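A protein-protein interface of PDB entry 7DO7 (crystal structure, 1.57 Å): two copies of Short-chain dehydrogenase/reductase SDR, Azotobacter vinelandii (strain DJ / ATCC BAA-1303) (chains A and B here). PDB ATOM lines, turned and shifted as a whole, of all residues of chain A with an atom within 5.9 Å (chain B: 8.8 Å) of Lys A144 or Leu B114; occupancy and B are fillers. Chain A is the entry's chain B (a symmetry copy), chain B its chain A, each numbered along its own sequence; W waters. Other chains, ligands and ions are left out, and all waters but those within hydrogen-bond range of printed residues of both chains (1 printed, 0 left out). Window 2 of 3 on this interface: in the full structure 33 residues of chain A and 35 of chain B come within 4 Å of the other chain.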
ATOM      1  N   VAL A 136      -7.071  18.106  20.503  1.00  0.00           N
ATOM      2  CA  VAL A 136      -8.311  18.842  20.267  1.00  0.00           C
ATOM      3  C   VAL A 136      -9.048  19.079  21.575  1.00  0.00           C
ATOM      4  O   VAL A 136      -9.542  20.184  21.831  1.00  0.00           O
ATOM      5  CB  VAL A 136      -9.183  18.081  19.247  1.00  0.00           C
ATOM      6  CG1 VAL A 136     -10.572  18.669  19.140  1.00  0.00           C
ATOM      7  CG2 VAL A 136      -8.509  18.108  17.886  1.00  0.00           C
ATOM      8  N   GLN A 137      -9.118  18.052  22.426  1.00  0.00           N
ATOM      9  CA  GLN A 137      -9.797  18.170  23.710  1.00  0.00           C
ATOM     10  C   GLN A 137      -9.171  19.265  24.570  1.00  0.00           C
ATOM     11  O   GLN A 137      -9.875  20.127  25.108  1.00  0.00           O
ATOM     12  CB  GLN A 137      -9.767  16.824  24.436  1.00  0.00           C
ATOM     13  CG  GLN A 137     -10.677  16.773  25.662  1.00  0.00           C
ATOM     14  CD  GLN A 137     -10.348  15.603  26.575  1.00  0.00           C
ATOM     15  OE1 GLN A 137      -9.253  15.530  27.136  1.00  0.00           O
ATOM     16  NE2 GLN A 137     -11.285  14.681  26.720  1.00  0.00           N
ATOM     17  N   ALA A 139      -7.294  21.848  23.679  1.00  0.00           N
ATOM     18  CA  ALA A 139      -7.482  23.167  23.093  1.00  0.00           C
ATOM     19  C   ALA A 139      -8.941  23.606  23.175  1.00  0.00           C
ATOM     20  O   ALA A 139      -9.223  24.781  23.422  1.00  0.00           O
ATOM     21  CB  ALA A 139      -6.991  23.169  21.647  1.00  0.00           C
ATOM     22  N   ALA A 140      -9.880  22.682  22.940  1.00  0.00           N
ATOM     23  CA  ALA A 140     -11.294  23.031  23.041  1.00  0.00           C
ATOM     24  C   ALA A 140     -11.671  23.393  24.466  1.00  0.00           C
ATOM     25  O   ALA A 140     -12.496  24.285  24.680  1.00  0.00           O
ATOM     26  CB  ALA A 140     -12.168  21.875  22.556  1.00  0.00           C
ATOM     27  N   ARG A 141     -11.113  22.676  25.449  1.00  0.00           N
ATOM     28  CA  ARG A 141     -11.377  23.016  26.844  1.00  0.00           C
ATOM     29  C   ARG A 141     -10.987  24.459  27.134  1.00  0.00           C
ATOM     30  O   ARG A 141     -11.718  25.184  27.818  1.00  0.00           O
ATOM     31  CB  ARG A 141     -10.618  22.056  27.759  1.00  0.00           C
ATOM     32  N   ARG A 142      -9.844  24.902  26.604  1.00  0.00           N
ATOM     33  CA  ARG A 142      -9.404  26.268  26.858  1.00  0.00           C
ATOM     34  C   ARG A 142     -10.275  27.278  26.117  1.00  0.00           C
ATOM     35  O   ARG A 142     -10.638  28.324  26.672  1.00  0.00           O
ATOM     36  CB  ARG A 142      -7.935  26.417  26.471  1.00  0.00           C
ATOM     37  CG  ARG A 142      -7.416  27.841  26.544  1.00  0.00           C
ATOM     38  CD  ARG A 142      -7.403  28.351  27.971  1.00  0.00           C
ATOM     39  NE  ARG A 142      -7.164  29.788  28.003  1.00  0.00           N
ATOM     40  CZ  ARG A 142      -6.739  30.455  29.075  1.00  0.00           C
ATOM     41  NH1 ARG A 142      -6.549  31.763  29.004  1.00  0.00           N
ATOM     42  NH2 ARG A 142      -6.506  29.810  30.209  1.00  0.00           N
ATOM     43  N   MET A 143     -10.611  26.990  24.856  1.00  0.00           N
ATOM     44  CA  MET A 143     -11.506  27.862  24.107  1.00  0.00           C
ATOM     45  C   MET A 143     -12.860  27.990  24.805  1.00  0.00           C
ATOM     46  O   MET A 143     -13.458  29.073  24.835  1.00  0.00           O
ATOM     47  CB  MET A 143     -11.681  27.326  22.682  1.00  0.00           C
ATOM     48  CG  MET A 143     -10.441  27.425  21.814  1.00  0.00           C
ATOM     49  SD  MET A 143     -10.728  26.435  20.326  1.00  0.00           S
ATOM     50  CE  MET A 143      -9.104  26.447  19.579  1.00  0.00           C
ATOM     51  N   LYS A 144     -13.365  26.891  25.361  1.00  0.00           N
ATOM     52  CA  LYS A 144     -14.636  26.965  26.066  1.00  0.00           C
ATOM     53  C   LYS A 144     -14.528  27.876  27.281  1.00  0.00           C
ATOM     54  O   LYS A 144     -15.405  28.711  27.522  1.00  0.00           O
ATOM     55  CB  LYS A 144     -15.085  25.572  26.484  1.00  0.00           C
ATOM     56  CG  LYS A 144     -16.410  25.571  27.210  1.00  0.00           C
ATOM     57  CD  LYS A 144     -16.727  24.197  27.745  1.00  0.00           C
ATOM     58  CE  LYS A 144     -18.034  24.214  28.535  1.00  0.00           C
ATOM     59  NZ  LYS A 144     -18.412  22.851  28.976  1.00  0.00           N
ATOM     60  N   GLU A 145     -13.438  27.743  28.040  1.00  0.00           N
ATOM     61  CA  GLU A 145     -13.274  28.545  29.248  1.00  0.00           C
ATOM     62  C   GLU A 145     -13.224  30.031  28.922  1.00  0.00           C
ATOM     63  O   GLU A 145     -13.771  30.860  29.659  1.00  0.00           O
ATOM     64  CB  GLU A 145     -12.009  28.109  29.981  1.00  0.00           C
ATOM     65  CG  GLU A 145     -11.488  29.133  30.988  1.00  0.00           C
ATOM     66  CD  GLU A 145     -10.287  28.626  31.763  1.00  0.00           C
ATOM     67  OE1 GLU A 145     -10.478  27.783  32.665  1.00  0.00           O
ATOM     68  OE2 GLU A 145      -9.156  29.072  31.467  1.00  0.00           O
ATOM     69  N   GLN A 146     -12.579  30.389  27.811  1.00  0.00           N
ATOM     70  CA  GLN A 146     -12.413  31.794  27.466  1.00  0.00           C
ATOM     71  C   GLN A 146     -13.733  32.447  27.085  1.00  0.00           C
ATOM     72  O   GLN A 146     -13.921  33.645  27.320  1.00  0.00           O
ATOM     73  CB  GLN A 146     -11.410  31.930  26.318  1.00  0.00           C
ATOM     74  CG  GLN A 146     -10.005  31.489  26.670  1.00  0.00           C
ATOM     75  CD  GLN A 146      -9.107  31.317  25.446  1.00  0.00           C
ATOM     76  OE1 GLN A 146      -7.914  31.074  25.583  1.00  0.00           O
ATOM     77  NE2 GLN A 146      -9.684  31.436  24.250  1.00  0.00           N
ATOM     78  N   GLY A 147     -14.647  31.692  26.485  1.00  0.00           N
ATOM     79  CA  GLY A 147     -15.921  32.251  26.080  1.00  0.00           C
ATOM     80  C   GLY A 147     -15.893  33.086  24.823  1.00  0.00           C
ATOM     81  O   GLY A 147     -16.847  33.834  24.577  1.00  0.00           O
ATOM     82  N   ARG A 148     -14.835  32.978  24.009  1.00  0.00           N
ATOM     83  CA  ARG A 148     -14.670  33.786  22.803  1.00  0.00           C
ATOM     84  C   ARG A 148     -14.826  32.979  21.514  1.00  0.00           C
ATOM     85  O   ARG A 148     -14.540  33.500  20.429  1.00  0.00           O
ATOM     86  CB  ARG A 148     -13.298  34.471  22.791  1.00  0.00           C
ATOM     87  CG  ARG A 148     -12.872  35.115  24.107  1.00  0.00           C
ATOM     88  CD  ARG A 148     -13.867  36.172  24.561  1.00  0.00           C
ATOM     89  NE  ARG A 148     -14.025  37.258  23.600  1.00  0.00           N
ATOM     90  CZ  ARG A 148     -13.184  38.280  23.469  1.00  0.00           C
ATOM     91  NH1 ARG A 148     -12.103  38.362  24.234  1.00  0.00           N
ATOM     92  NH2 ARG A 148     -13.420  39.220  22.561  1.00  0.00           N
ATOM     93  N   LEU A 188     -19.224  21.161  20.293  1.00  0.00           N
ATOM     94  CA  LEU A 188     -18.633  22.448  20.631  1.00  0.00           C
ATOM     95  C   LEU A 188     -19.316  23.638  19.975  1.00  0.00           C
ATOM     96  O   LEU A 188     -18.964  24.783  20.293  1.00  0.00           O
ATOM     97  CB  LEU A 188     -17.145  22.464  20.263  1.00  0.00           C
ATOM     98  CG  LEU A 188     -16.302  21.327  20.824  1.00  0.00           C
ATOM     99  CD1 LEU A 188     -14.899  21.449  20.270  1.00  0.00           C
ATOM    100  CD2 LEU A 188     -16.275  21.415  22.331  1.00  0.00           C
ATOM    101  N   TYR A 191     -20.508  26.483  22.012  1.00  0.00           N
ATOM    102  CA  TYR A 191     -19.454  27.338  22.539  1.00  0.00           C
ATOM    103  C   TYR A 191     -18.726  28.100  21.437  1.00  0.00           C
ATOM    104  O   TYR A 191     -17.659  28.670  21.690  1.00  0.00           O
ATOM    105  CB  TYR A 191     -18.471  26.504  23.356  1.00  0.00           C
ATOM    106  CG  TYR A 191     -19.153  25.598  24.330  1.00  0.00           C
ATOM    107  CD1 TYR A 191     -19.912  26.123  25.366  1.00  0.00           C
ATOM    108  CD2 TYR A 191     -19.067  24.220  24.208  1.00  0.00           C
ATOM    109  CE1 TYR A 191     -20.555  25.302  26.263  1.00  0.00           C
ATOM    110  CE2 TYR A 191     -19.710  23.387  25.101  1.00  0.00           C
ATOM    111  CZ  TYR A 191     -20.455  23.938  26.130  1.00  0.00           C
ATOM    112  OH  TYR A 191     -21.093  23.122  27.034  1.00  0.00           O
ATOM    113  N   ILE A 193     -17.077  27.144  18.818  1.00  0.00           N
ATOM    114  CA  ILE A 193     -15.828  26.551  18.347  1.00  0.00           C
ATOM    115  C   ILE A 193     -16.155  25.789  17.074  1.00  0.00           C
ATOM    116  O   ILE A 193     -16.870  24.783  17.105  1.00  0.00           O
ATOM    117  CB  ILE A 193     -15.185  25.643  19.400  1.00  0.00           C
ATOM    118  CG1 ILE A 193     -14.974  26.428  20.704  1.00  0.00           C
ATOM    119  CG2 ILE A 193     -13.866  25.057  18.878  1.00  0.00           C
ATOM    120  CD1 ILE A 193     -14.720  25.556  21.930  1.00  0.00           C
ATOM    121  N   HIS B 111     -20.717   9.313  25.869  1.00  0.00           N
ATOM    122  CA  HIS B 111     -19.947  10.113  26.804  1.00  0.00           C
ATOM    123  C   HIS B 111     -19.615  11.451  26.159  1.00  0.00           C
ATOM    124  O   HIS B 111     -19.387  11.526  24.948  1.00  0.00           O
ATOM    125  CB  HIS B 111     -18.673   9.371  27.224  1.00  0.00           C
ATOM    126  CG  HIS B 111     -18.092   9.850  28.515  1.00  0.00           C
ATOM    127  ND1 HIS B 111     -17.410  11.041  28.624  1.00  0.00           N
ATOM    128  CD2 HIS B 111     -18.078   9.291  29.750  1.00  0.00           C
ATOM    129  CE1 HIS B 111     -17.013  11.204  29.874  1.00  0.00           C
ATOM    130  NE2 HIS B 111     -17.409  10.158  30.578  1.00  0.00           N
ATOM    131  N   SER B 112     -19.594  12.500  26.971  1.00  0.00           N
ATOM    132  CA  SER B 112     -19.259  13.812  26.445  1.00  0.00           C
ATOM    133  C   SER B 112     -17.769  13.896  26.129  1.00  0.00           C
ATOM    134  O   SER B 112     -16.954  13.090  26.593  1.00  0.00           O
ATOM    135  CB  SER B 112     -19.672  14.909  27.428  1.00  0.00           C
ATOM    136  OG  SER B 112     -19.415  14.506  28.764  1.00  0.00           O
ATOM    137  N   PHE B 113     -17.429  14.903  25.323  1.00  0.00           N
ATOM    138  CA  PHE B 113     -16.106  14.989  24.717  1.00  0.00           C
ATOM    139  C   PHE B 113     -15.087  15.601  25.674  1.00  0.00           C
ATOM    140  O   PHE B 113     -13.982  15.075  25.832  1.00  0.00           O
ATOM    141  CB  PHE B 113     -16.198  15.800  23.420  1.00  0.00           C
ATOM    142  CG  PHE B 113     -14.872  16.164  22.836  1.00  0.00           C
ATOM    143  CD1 PHE B 113     -13.996  15.175  22.430  1.00  0.00           C
ATOM    144  CD2 PHE B 113     -14.501  17.492  22.678  1.00  0.00           C
ATOM    145  CE1 PHE B 113     -12.752  15.499  21.868  1.00  0.00           C
ATOM    146  CE2 PHE B 113     -13.257  17.818  22.138  1.00  0.00           C
ATOM    147  CZ  PHE B 113     -12.394  16.820  21.735  1.00  0.00           C
ATOM    148  N   LEU B 114     -15.447  16.703  26.333  1.00  0.00           N
ATOM    149  CA  LEU B 114     -14.440  17.455  27.075  1.00  0.00           C
ATOM    150  C   LEU B 114     -13.940  16.719  28.312  1.00  0.00           C
ATOM    151  O   LEU B 114     -12.820  16.987  28.760  1.00  0.00           O
ATOM    152  CB  LEU B 114     -14.992  18.827  27.460  1.00  0.00           C
ATOM    153  CG  LEU B 114     -15.269  19.755  26.274  1.00  0.00           C
ATOM    154  CD1 LEU B 114     -15.948  21.024  26.717  1.00  0.00           C
ATOM    155  CD2 LEU B 114     -13.997  20.106  25.522  1.00  0.00           C
ATOM    156  N   ASP B 115     -14.732  15.805  28.871  1.00  0.00           N
ATOM    157  CA  ASP B 115     -14.311  15.018  30.021  1.00  0.00           C
ATOM    158  C   ASP B 115     -14.117  13.545  29.677  1.00  0.00           C
ATOM    159  O   ASP B 115     -14.073  12.701  30.575  1.00  0.00           O
ATOM    160  CB  ASP B 115     -15.314  15.178  31.169  1.00  0.00           C
ATOM    161  CG  ASP B 115     -16.739  14.868  30.749  1.00  0.00           C
ATOM    162  OD1 ASP B 115     -16.998  14.781  29.531  1.00  0.00           O
ATOM    163  OD2 ASP B 115     -17.605  14.704  31.633  1.00  0.00           O
ATOM    164  N   MET B 116     -13.984  13.220  28.394  1.00  0.00           N
ATOM    165  CA  MET B 116     -13.778  11.848  27.966  1.00  0.00           C
ATOM    166  C   MET B 116     -12.555  11.235  28.648  1.00  0.00           C
ATOM    167  O   MET B 116     -11.440  11.750  28.479  1.00  0.00           O
ATOM    168  CB  MET B 116     -13.596  11.802  26.452  1.00  0.00           C
ATOM    169  CG  MET B 116     -13.213  10.427  25.928  1.00  0.00           C
ATOM    170  SD  MET B 116     -14.548   9.229  26.099  1.00  0.00           S
ATOM    171  CE  MET B 116     -15.819  10.050  25.145  1.00  0.00           C
ATOM    172  N   PRO B 117     -12.716  10.145  29.402  1.00  0.00           N
ATOM    173  CA  PRO B 117     -11.546   9.483  29.996  1.00  0.00           C
ATOM    174  C   PRO B 117     -10.669   8.841  28.928  1.00  0.00           C
ATOM    175  O   PRO B 117     -11.164   8.328  27.924  1.00  0.00           O
ATOM    176  CB  PRO B 117     -12.166   8.427  30.921  1.00  0.00           C
ATOM    177  CG  PRO B 117     -13.601   8.882  31.140  1.00  0.00           C
ATOM    178  CD  PRO B 117     -13.984   9.546  29.852  1.00  0.00           C
ATOM    179  N   ALA B 165     -22.655  14.192  19.198  1.00  0.00           N
ATOM    180  CA  ALA B 165     -21.995  14.971  20.244  1.00  0.00           C
ATOM    181  C   ALA B 165     -21.433  14.075  21.346  1.00  0.00           C
ATOM    182  O   ALA B 165     -20.348  14.346  21.882  1.00  0.00           O
ATOM    183  CB  ALA B 165     -22.968  15.997  20.826  1.00  0.00           C
ATOM    184  N   MET B 166     -22.161  13.013  21.703  1.00  0.00           N
ATOM    185  CA  MET B 166     -21.754  12.053  22.722  1.00  0.00           C
ATOM    186  C   MET B 166     -21.037  10.855  22.131  1.00  0.00           C
ATOM    187  O   MET B 166     -20.920   9.814  22.794  1.00  0.00           O
ATOM    188  CB  MET B 166     -22.976  11.605  23.527  1.00  0.00           C
ATOM    189  CG  MET B 166     -23.729  12.788  24.097  1.00  0.00           C
ATOM    190  SD  MET B 166     -22.795  13.539  25.436  1.00  0.00           S
ATOM    191  CE  MET B 166     -23.045  12.319  26.727  1.00  0.00           C
ATOM    192  N   THR B 168     -17.961  11.353  20.103  1.00  0.00           N
ATOM    193  CA  THR B 168     -16.719  11.842  19.499  1.00  0.00           C
ATOM    194  C   THR B 168     -15.645  10.763  19.471  1.00  0.00           C
ATOM    195  O   THR B 168     -14.780  10.783  18.594  1.00  0.00           O
ATOM    196  CB  THR B 168     -16.166  13.058  20.240  1.00  0.00           C
ATOM    197  OG1 THR B 168     -15.916  12.714  21.608  1.00  0.00           O
ATOM    198  CG2 THR B 168     -17.112  14.242  20.146  1.00  0.00           C
HETATM  199  O   HOH W   1      -9.675  13.389  29.554  1.00  0.00           O
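The side-chain amide nitrogen of Gln A137 sits at hydrogen-bond distance from the backbone carbonyl oxygen of Leu B114, at 3.4 Å. The backbone carbonyl oxygen of Met B116 lies within hydrogen-bond range of the side-chain amide nitrogen of Gln A137, at 3.4 Å. The backbone carbonyl oxygen of Phe B113 sits at hydrogen-bond distance from the side-chain amide nitrogen of Gln A137 (2.9 Å).
NZ of Lys A144 is in hydrogen-bond range of OH of Tyr A191, at 3.3 Å.
Among the printed residues, pairs that only touch across the chains: Lys A144 with Leu B114, Val A136 with Phe B113, Arg A141 with Leu B114 and Ala A140 with Leu B114.
Printed residues of chain B within 4 Å of Lys A144: Leu B114. Arg A141 touches just one residue of chain B: Leu B114 (3.9 Å). Printed residues of chain B within 4 Å of Ala A140: Leu B114. Of the printed residues of chain B, Val A136 touches Phe B113 (3.7 Å). His B111 touches none of the printed residues of chain A. The nearest residue of chain A that does not touch Leu B114 is Leu A188 (4.1 Å).
Of the 15 printed residues of chain A, 5 touch a printed residue of chain B. Hydrophobic or aromatic side chains of chain A within 4 Å of the printed part of chain B: Val A136 and Ala A140. Printed residues of chain B that touch a printed residue of chain A: Phe B113, Leu B114 and Met B116.
No position is printed for both chains. Of the 7 pairs that touch across the chains among the printed residues, none has its exchanged pair printed and touching as well.
Water W1 lies within hydrogen-bond range of the backbone carbonyl oxygen (O) of Met B116 (2.6 Å) and the side-chain amide oxygen (OE1) of Gln A137 (3.3 Å).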
